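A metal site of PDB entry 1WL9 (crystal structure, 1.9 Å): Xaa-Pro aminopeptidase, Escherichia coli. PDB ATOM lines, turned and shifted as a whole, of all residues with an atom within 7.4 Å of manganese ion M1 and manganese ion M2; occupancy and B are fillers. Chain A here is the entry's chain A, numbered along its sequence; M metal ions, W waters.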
ATOM      1  N   TYR A 229      -0.505  -7.593 -15.664  1.00  0.00           N
ATOM      2  CA  TYR A 229      -1.287  -6.562 -16.376  1.00  0.00           C
ATOM      3  C   TYR A 229      -0.475  -6.148 -17.585  1.00  0.00           C
ATOM      4  O   TYR A 229       0.701  -6.462 -17.666  1.00  0.00           O
ATOM      5  CB  TYR A 229      -1.576  -5.318 -15.512  1.00  0.00           C
ATOM      6  CG  TYR A 229      -0.346  -4.719 -14.863  1.00  0.00           C
ATOM      7  CD1 TYR A 229       0.112  -5.163 -13.624  1.00  0.00           C
ATOM      8  CD2 TYR A 229       0.375  -3.705 -15.506  1.00  0.00           C
ATOM      9  CE1 TYR A 229       1.228  -4.626 -13.047  1.00  0.00           C
ATOM     10  CE2 TYR A 229       1.519  -3.160 -14.919  1.00  0.00           C
ATOM     11  CZ  TYR A 229       1.928  -3.612 -13.680  1.00  0.00           C
ATOM     12  OH  TYR A 229       3.058  -3.048 -13.102  1.00  0.00           O
ATOM     13  N   ILE A 232       3.294  -1.073 -19.507  1.00  0.00           N
ATOM     14  CA  ILE A 232       3.302   0.316 -19.959  1.00  0.00           C
ATOM     15  C   ILE A 232       4.735   0.783 -20.088  1.00  0.00           C
ATOM     16  O   ILE A 232       5.492   0.713 -19.115  1.00  0.00           O
ATOM     17  CB  ILE A 232       2.620   1.204 -18.906  1.00  0.00           C
ATOM     18  CG1 ILE A 232       1.135   0.832 -18.813  1.00  0.00           C
ATOM     19  CG2 ILE A 232       2.810   2.695 -19.195  1.00  0.00           C
ATOM     20  CD1 ILE A 232       0.488   1.321 -17.537  1.00  0.00           C
ATOM     21  N   HIS A 243      -2.427   4.694 -18.699  1.00  0.00           N
ATOM     22  CA  HIS A 243      -2.280   3.282 -19.129  1.00  0.00           C
ATOM     23  C   HIS A 243      -1.942   3.233 -20.635  1.00  0.00           C
ATOM     24  O   HIS A 243      -2.645   2.637 -21.436  1.00  0.00           O
ATOM     25  CB  HIS A 243      -3.511   2.430 -18.777  1.00  0.00           C
ATOM     26  CG  HIS A 243      -3.868   2.446 -17.313  1.00  0.00           C
ATOM     27  ND1 HIS A 243      -2.966   2.785 -16.323  1.00  0.00           N
ATOM     28  CD2 HIS A 243      -5.026   2.154 -16.678  1.00  0.00           C
ATOM     29  CE1 HIS A 243      -3.559   2.708 -15.142  1.00  0.00           C
ATOM     30  NE2 HIS A 243      -4.805   2.314 -15.331  1.00  0.00           N
ATOM     31  N   ILE A 259       8.057   3.267 -16.971  1.00  0.00           N
ATOM     32  CA  ILE A 259       7.776   1.841 -17.139  1.00  0.00           C
ATOM     33  C   ILE A 259       6.958   1.351 -15.954  1.00  0.00           C
ATOM     34  O   ILE A 259       7.418   1.417 -14.803  1.00  0.00           O
ATOM     35  CB  ILE A 259       9.047   1.017 -17.252  1.00  0.00           C
ATOM     36  CG1 ILE A 259       9.877   1.489 -18.458  1.00  0.00           C
ATOM     37  CG2 ILE A 259       8.698  -0.454 -17.402  1.00  0.00           C
ATOM     38  CD1 ILE A 259      11.066   0.602 -18.743  1.00  0.00           C
ATOM     39  N   ASP A 260       5.759   0.857 -16.238  1.00  0.00           N
ATOM     40  CA  ASP A 260       4.898   0.250 -15.237  1.00  0.00           C
ATOM     41  C   ASP A 260       4.682  -1.187 -15.686  1.00  0.00           C
ATOM     42  O   ASP A 260       4.081  -1.465 -16.735  1.00  0.00           O
ATOM     43  CB  ASP A 260       3.591   1.025 -15.086  1.00  0.00           C
ATOM     44  CG  ASP A 260       2.789   0.627 -13.867  1.00  0.00           C
ATOM     45  OD1 ASP A 260       3.009  -0.458 -13.273  1.00  0.00           O
ATOM     46  OD2 ASP A 260       1.904   1.420 -13.468  1.00  0.00           O
ATOM     47  N   ALA A 261       5.282  -2.113 -14.948  1.00  0.00           N
ATOM     48  CA  ALA A 261       5.205  -3.525 -15.298  1.00  0.00           C
ATOM     49  C   ALA A 261       5.340  -4.398 -14.074  1.00  0.00           C
ATOM     50  O   ALA A 261       6.005  -4.037 -13.092  1.00  0.00           O
ATOM     51  CB  ALA A 261       6.285  -3.888 -16.320  1.00  0.00           C
ATOM     52  N   GLY A 262       4.670  -5.536 -14.138  1.00  0.00           N
ATOM     53  CA  GLY A 262       4.619  -6.455 -13.025  1.00  0.00           C
ATOM     54  C   GLY A 262       4.394  -7.865 -13.483  1.00  0.00           C
ATOM     55  O   GLY A 262       3.659  -8.122 -14.450  1.00  0.00           O
ATOM     56  N   GLY A 270       3.083  -8.768  -8.989  1.00  0.00           N
ATOM     57  CA  GLY A 270       3.929  -7.603  -8.775  1.00  0.00           C
ATOM     58  C   GLY A 270       3.373  -6.396  -9.512  1.00  0.00           C
ATOM     59  O   GLY A 270       2.591  -6.527 -10.473  1.00  0.00           O
ATOM     60  N   ASP A 271       3.787  -5.206  -9.094  1.00  0.00           N
ATOM     61  CA  ASP A 271       3.331  -3.965  -9.700  1.00  0.00           C
ATOM     62  C   ASP A 271       4.321  -2.834  -9.368  1.00  0.00           C
ATOM     63  O   ASP A 271       4.225  -2.205  -8.340  1.00  0.00           O
ATOM     64  CB  ASP A 271       1.931  -3.631  -9.176  1.00  0.00           C
ATOM     65  CG  ASP A 271       1.331  -2.404  -9.832  1.00  0.00           C
ATOM     66  OD1 ASP A 271       1.969  -1.797 -10.751  1.00  0.00           O
ATOM     67  OD2 ASP A 271       0.198  -2.068  -9.430  1.00  0.00           O
ATOM     68  N   ILE A 272       5.279  -2.609 -10.265  1.00  0.00           N
ATOM     69  CA  ILE A 272       6.315  -1.598 -10.089  1.00  0.00           C
ATOM     70  C   ILE A 272       6.264  -0.592 -11.207  1.00  0.00           C
ATOM     71  O   ILE A 272       6.072  -0.943 -12.392  1.00  0.00           O
ATOM     72  CB  ILE A 272       7.710  -2.233 -10.064  1.00  0.00           C
ATOM     73  CG1 ILE A 272       7.898  -3.134  -8.832  1.00  0.00           C
ATOM     74  CG2 ILE A 272       8.813  -1.145 -10.145  1.00  0.00           C
ATOM     75  CD1 ILE A 272       9.263  -3.722  -8.745  1.00  0.00           C
ATOM     76  N   THR A 273       6.392   0.679 -10.824  1.00  0.00           N
ATOM     77  CA  THR A 273       6.652   1.732 -11.792  1.00  0.00           C
ATOM     78  C   THR A 273       8.010   2.378 -11.453  1.00  0.00           C
ATOM     79  O   THR A 273       8.308   2.696 -10.291  1.00  0.00           O
ATOM     80  CB  THR A 273       5.562   2.829 -11.840  1.00  0.00           C
ATOM     81  OG1 THR A 273       4.243   2.268 -11.995  1.00  0.00           O
ATOM     82  CG2 THR A 273       5.814   3.747 -13.004  1.00  0.00           C
ATOM     83  N   GLY A 351      -5.343   7.554  -7.511  1.00  0.00           N
ATOM     84  CA  GLY A 351      -5.133   7.166  -6.127  1.00  0.00           C
ATOM     85  C   GLY A 351      -3.683   6.841  -5.839  1.00  0.00           C
ATOM     86  O   GLY A 351      -2.921   6.447  -6.741  1.00  0.00           O
ATOM     87  N   LEU A 352      -3.295   7.042  -4.582  1.00  0.00           N
ATOM     88  CA  LEU A 352      -1.932   6.757  -4.132  1.00  0.00           C
ATOM     89  C   LEU A 352      -1.658   5.257  -4.006  1.00  0.00           C
ATOM     90  O   LEU A 352      -0.539   4.797  -4.203  1.00  0.00           O
ATOM     91  CB  LEU A 352      -1.677   7.417  -2.765  1.00  0.00           C
ATOM     92  CG  LEU A 352      -0.284   7.222  -2.141  1.00  0.00           C
ATOM     93  CD1 LEU A 352       0.780   7.909  -2.999  1.00  0.00           C
ATOM     94  CD2 LEU A 352      -0.232   7.725  -0.709  1.00  0.00           C
ATOM     95  N   SER A 353      -2.687   4.492  -3.642  1.00  0.00           N
ATOM     96  CA  SER A 353      -2.485   3.099  -3.271  1.00  0.00           C
ATOM     97  C   SER A 353      -3.694   2.262  -3.600  1.00  0.00           C
ATOM     98  O   SER A 353      -4.822   2.705  -3.414  1.00  0.00           O
ATOM     99  CB  SER A 353      -2.239   3.014  -1.765  1.00  0.00           C
ATOM    100  OG  SER A 353      -1.029   3.633  -1.366  1.00  0.00           O
ATOM    101  N   HIS A 354      -3.460   1.042  -4.063  1.00  0.00           N
ATOM    102  CA  HIS A 354      -4.504   0.033  -4.179  1.00  0.00           C
ATOM    103  C   HIS A 354      -3.995  -1.259  -3.546  1.00  0.00           C
ATOM    104  O   HIS A 354      -2.790  -1.504  -3.473  1.00  0.00           O
ATOM    105  CB  HIS A 354      -4.933  -0.196  -5.617  1.00  0.00           C
ATOM    106  CG  HIS A 354      -3.818  -0.604  -6.522  1.00  0.00           C
ATOM    107  ND1 HIS A 354      -3.367  -1.905  -6.619  1.00  0.00           N
ATOM    108  CD2 HIS A 354      -3.061   0.119  -7.377  1.00  0.00           C
ATOM    109  CE1 HIS A 354      -2.368  -1.951  -7.478  1.00  0.00           C
ATOM    110  NE2 HIS A 354      -2.170  -0.738  -7.959  1.00  0.00           N
ATOM    111  N   TRP A 355      -4.907  -2.067  -3.064  1.00  0.00           N
ATOM    112  CA  TRP A 355      -4.579  -3.416  -2.612  1.00  0.00           C
ATOM    113  C   TRP A 355      -3.945  -4.219  -3.750  1.00  0.00           C
ATOM    114  O   TRP A 355      -4.250  -4.003  -4.941  1.00  0.00           O
ATOM    115  CB  TRP A 355      -5.800  -4.210  -2.147  1.00  0.00           C
ATOM    116  CG  TRP A 355      -6.763  -3.531  -1.232  1.00  0.00           C
ATOM    117  CD1 TRP A 355      -8.100  -3.427  -1.430  1.00  0.00           C
ATOM    118  CD2 TRP A 355      -6.500  -2.917   0.053  1.00  0.00           C
ATOM    119  NE1 TRP A 355      -8.696  -2.764  -0.377  1.00  0.00           N
ATOM    120  CE2 TRP A 355      -7.742  -2.450   0.551  1.00  0.00           C
ATOM    121  CE3 TRP A 355      -5.347  -2.734   0.825  1.00  0.00           C
ATOM    122  CZ2 TRP A 355      -7.867  -1.802   1.790  1.00  0.00           C
ATOM    123  CZ3 TRP A 355      -5.463  -2.068   2.054  1.00  0.00           C
ATOM    124  CH2 TRP A 355      -6.714  -1.617   2.531  1.00  0.00           C
ATOM    125  N   LEU A 356      -3.134  -5.197  -3.356  1.00  0.00           N
ATOM    126  CA  LEU A 356      -2.383  -6.047  -4.267  1.00  0.00           C
ATOM    127  C   LEU A 356      -2.469  -7.519  -3.838  1.00  0.00           C
ATOM    128  O   LEU A 356      -2.394  -7.852  -2.632  1.00  0.00           O
ATOM    129  CB  LEU A 356      -0.927  -5.585  -4.267  1.00  0.00           C
ATOM    130  CG  LEU A 356       0.032  -6.201  -5.289  1.00  0.00           C
ATOM    131  CD1 LEU A 356      -0.297  -5.738  -6.719  1.00  0.00           C
ATOM    132  CD2 LEU A 356       1.431  -5.825  -4.922  1.00  0.00           C
ATOM    133  N   VAL A 360      -3.991  -7.475  -9.562  1.00  0.00           N
ATOM    134  CA  VAL A 360      -3.194  -6.273  -9.376  1.00  0.00           C
ATOM    135  C   VAL A 360      -4.002  -5.193  -8.695  1.00  0.00           C
ATOM    136  O   VAL A 360      -3.494  -4.544  -7.800  1.00  0.00           O
ATOM    137  CB  VAL A 360      -2.521  -5.771 -10.681  1.00  0.00           C
ATOM    138  CG1 VAL A 360      -3.507  -5.421 -11.751  1.00  0.00           C
ATOM    139  CG2 VAL A 360      -1.624  -4.557 -10.385  1.00  0.00           C
ATOM    140  N   HIS A 361      -5.254  -5.000  -9.100  1.00  0.00           N
ATOM    141  CA  HIS A 361      -6.167  -4.175  -8.289  1.00  0.00           C
ATOM    142  C   HIS A 361      -6.944  -5.135  -7.424  1.00  0.00           C
ATOM    143  O   HIS A 361      -8.009  -5.628  -7.798  1.00  0.00           O
ATOM    144  CB  HIS A 361      -7.081  -3.307  -9.128  1.00  0.00           C
ATOM    145  CG  HIS A 361      -6.348  -2.303  -9.941  1.00  0.00           C
ATOM    146  ND1 HIS A 361      -6.797  -1.865 -11.161  1.00  0.00           N
ATOM    147  CD2 HIS A 361      -5.139  -1.721  -9.744  1.00  0.00           C
ATOM    148  CE1 HIS A 361      -5.911  -1.019 -11.671  1.00  0.00           C
ATOM    149  NE2 HIS A 361      -4.906  -0.909 -10.822  1.00  0.00           N
ATOM    150  N   THR A 381      -0.039  -1.047  -2.960  1.00  0.00           N
ATOM    151  CA  THR A 381       0.960  -0.296  -3.696  1.00  0.00           C
ATOM    152  C   THR A 381       1.083   1.106  -3.137  1.00  0.00           C
ATOM    153  O   THR A 381       0.218   1.571  -2.391  1.00  0.00           O
ATOM    154  CB  THR A 381       0.612  -0.192  -5.210  1.00  0.00           C
ATOM    155  OG1 THR A 381      -0.613   0.540  -5.362  1.00  0.00           O
ATOM    156  CG2 THR A 381       0.485  -1.557  -5.807  1.00  0.00           C
ATOM    157  N   VAL A 382       2.190   1.762  -3.476  1.00  0.00           N
ATOM    158  CA  VAL A 382       2.387   3.170  -3.158  1.00  0.00           C
ATOM    159  C   VAL A 382       2.925   3.798  -4.456  1.00  0.00           C
ATOM    160  O   VAL A 382       4.045   3.503  -4.866  1.00  0.00           O
ATOM    161  CB  VAL A 382       3.382   3.351  -1.975  1.00  0.00           C
ATOM    162  CG1 VAL A 382       3.420   4.812  -1.494  1.00  0.00           C
ATOM    163  CG2 VAL A 382       3.054   2.395  -0.833  1.00  0.00           C
ATOM    164  N   GLU A 383       2.123   4.634  -5.097  1.00  0.00           N
ATOM    165  CA  GLU A 383       2.415   5.076  -6.451  1.00  0.00           C
ATOM    166  C   GLU A 383       2.050   6.539  -6.738  1.00  0.00           C
ATOM    167  O   GLU A 383       1.235   6.838  -7.601  1.00  0.00           O
ATOM    168  CB  GLU A 383       1.778   4.139  -7.478  1.00  0.00           C
ATOM    169  CG  GLU A 383       0.272   3.925  -7.397  1.00  0.00           C
ATOM    170  CD  GLU A 383      -0.197   2.923  -8.437  1.00  0.00           C
ATOM    171  OE1 GLU A 383       0.120   3.099  -9.643  1.00  0.00           O
ATOM    172  OE2 GLU A 383      -0.848   1.950  -8.044  1.00  0.00           O
ATOM    173  N   ARG A 404       5.883   8.598 -12.560  1.00  0.00           N
ATOM    174  CA  ARG A 404       5.342   7.821 -11.458  1.00  0.00           C
ATOM    175  C   ARG A 404       6.429   6.909 -10.913  1.00  0.00           C
ATOM    176  O   ARG A 404       7.297   6.408 -11.650  1.00  0.00           O
ATOM    177  CB  ARG A 404       4.098   7.030 -11.914  1.00  0.00           C
ATOM    178  CG  ARG A 404       3.554   6.078 -10.890  1.00  0.00           C
ATOM    179  CD  ARG A 404       2.175   5.546 -11.294  1.00  0.00           C
ATOM    180  NE  ARG A 404       2.145   4.637 -12.443  1.00  0.00           N
ATOM    181  CZ  ARG A 404       1.716   4.942 -13.679  1.00  0.00           C
ATOM    182  NH1 ARG A 404       1.343   6.152 -14.006  1.00  0.00           N
ATOM    183  NH2 ARG A 404       1.670   4.010 -14.619  1.00  0.00           N
ATOM    184  N   GLU A 406       6.534   3.658  -8.157  1.00  0.00           N
ATOM    185  CA  GLU A 406       5.613   2.757  -7.469  1.00  0.00           C
ATOM    186  C   GLU A 406       6.338   1.557  -6.883  1.00  0.00           C
ATOM    187  O   GLU A 406       7.061   0.861  -7.608  1.00  0.00           O
ATOM    188  CB  GLU A 406       4.526   2.276  -8.433  1.00  0.00           C
ATOM    189  CG  GLU A 406       3.680   1.096  -7.957  1.00  0.00           C
ATOM    190  CD  GLU A 406       2.547   0.786  -8.924  1.00  0.00           C
ATOM    191  OE1 GLU A 406       2.765   0.945 -10.130  1.00  0.00           O
ATOM    192  OE2 GLU A 406       1.448   0.402  -8.463  1.00  0.00           O
ATOM    193  N   ASP A 407       6.102   1.336  -5.590  1.00  0.00           N
ATOM    194  CA  ASP A 407       6.586   0.188  -4.841  1.00  0.00           C
ATOM    195  C   ASP A 407       5.398  -0.592  -4.306  1.00  0.00           C
ATOM    196  O   ASP A 407       4.306  -0.051  -4.206  1.00  0.00           O
ATOM    197  CB  ASP A 407       7.459   0.636  -3.676  1.00  0.00           C
ATOM    198  CG  ASP A 407       8.901   0.942  -4.102  1.00  0.00           C
ATOM    199  OD1 ASP A 407       9.369   0.354  -5.101  1.00  0.00           O
ATOM    200  OD2 ASP A 407       9.530   1.726  -3.393  1.00  0.00           O
ATOM    201  N   ASP A 408       5.632  -1.854  -3.960  1.00  0.00           N
ATOM    202  CA  ASP A 408       4.627  -2.720  -3.339  1.00  0.00           C
ATOM    203  C   ASP A 408       5.053  -2.998  -1.892  1.00  0.00           C
ATOM    204  O   ASP A 408       6.226  -3.335  -1.623  1.00  0.00           O
ATOM    205  CB  ASP A 408       4.504  -4.048  -4.095  1.00  0.00           C
ATOM    206  CG  ASP A 408       4.327  -3.853  -5.567  1.00  0.00           C
ATOM    207  OD1 ASP A 408       3.686  -2.830  -5.941  1.00  0.00           O
ATOM    208  OD2 ASP A 408       4.828  -4.715  -6.337  1.00  0.00           O
HETATM  209 MN    MN M   1      -0.521   0.009  -9.169  1.00  0.00          MN
HETATM  210 MN    MN M   2       1.568   0.004 -11.704  1.00  0.00          MN
HETATM  211  O   HOH W   1      -0.193   0.956 -10.952  1.00  0.00           O
HETATM  212  O   HOH W   2      -2.485  -0.280 -11.201  1.00  0.00           O
HETATM  213  O   HOH W   3      -0.239  -1.078 -12.819  1.00  0.00           O
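N of Asp 271 is in hydrogen-bond range of OD2 of Asp 408 (3.0 Å). O of His 354 is in hydrogen-bond range of N of Thr 381, at 2.8 Å. A ring nitrogen (ND1) of His 354 lies close to the backbone carbonyl oxygen of Val 360 (2.9 Å). N of Asp 260 lies within hydrogen-bond range of O of Ile 232, 2.9 Å away. The side-chain carboxylate (OE1) of Glu 383 lies within salt-bridge range of the guanidinium group (NE) of Arg 404, at 3.8 Å. The side-chain hydroxyl (OG1) of Thr 273 is in hydrogen-bond range of the guanidinium group (NE) of Arg 404, 3.2 Å away. The side-chain hydroxyl (OH) of Tyr 229 sits close to the backbone NH (N) of Ala 261. The side-chain hydroxyl of Tyr 229 is in hydrogen-bond range of the backbone NH of Gly 262 (3.1 Å).
CG2 of Thr 381 touches manganese ion M1 (3.8 Å). Of the 26 residues printed, 5 come within 4 Å of manganese ion M1. Along chain A the residues within 4 Å of manganese ion M1 span positions 271 to 406. The nearest printed residue that does not touch manganese ion M1 is His 361 (4.8 Å).
Tyr 229 touches manganese ion M2 (OH to MN, 3.7 Å). Thr 273 touches manganese ion M2 (OG1 to MN, 3.5 Å). Six residues have an atom within 4 Å of manganese ion M2: Tyr 229, Asp 260, Asp 271, Thr 273, Glu 383 and Glu 406.
Manganese ion M1 is bound by water W1, the side-chain carboxylate of Glu 406, a ring nitrogen (NE2) of His 354, the side-chain carboxylate of Asp 271 and the side-chain carboxylate of Glu 383. Slightly farther from manganese ion M1 lies water W2 (2.8 Å).
Manganese ion M2 is bound by the side-chain carboxylate (OD1) of Asp 271 (2.1 Å), water W1 (2.1 Å), the side-chain carboxylate (OD1) of Asp 260 (2.2 Å), the side-chain carboxylate (OE1) of Glu 406 (2.2 Å), the side-chain carboxylate (OD2) of Asp 260 (2.3 Å) and water W3 (2.4 Å). Manganese ion M2 has six donor atoms within binding distance.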
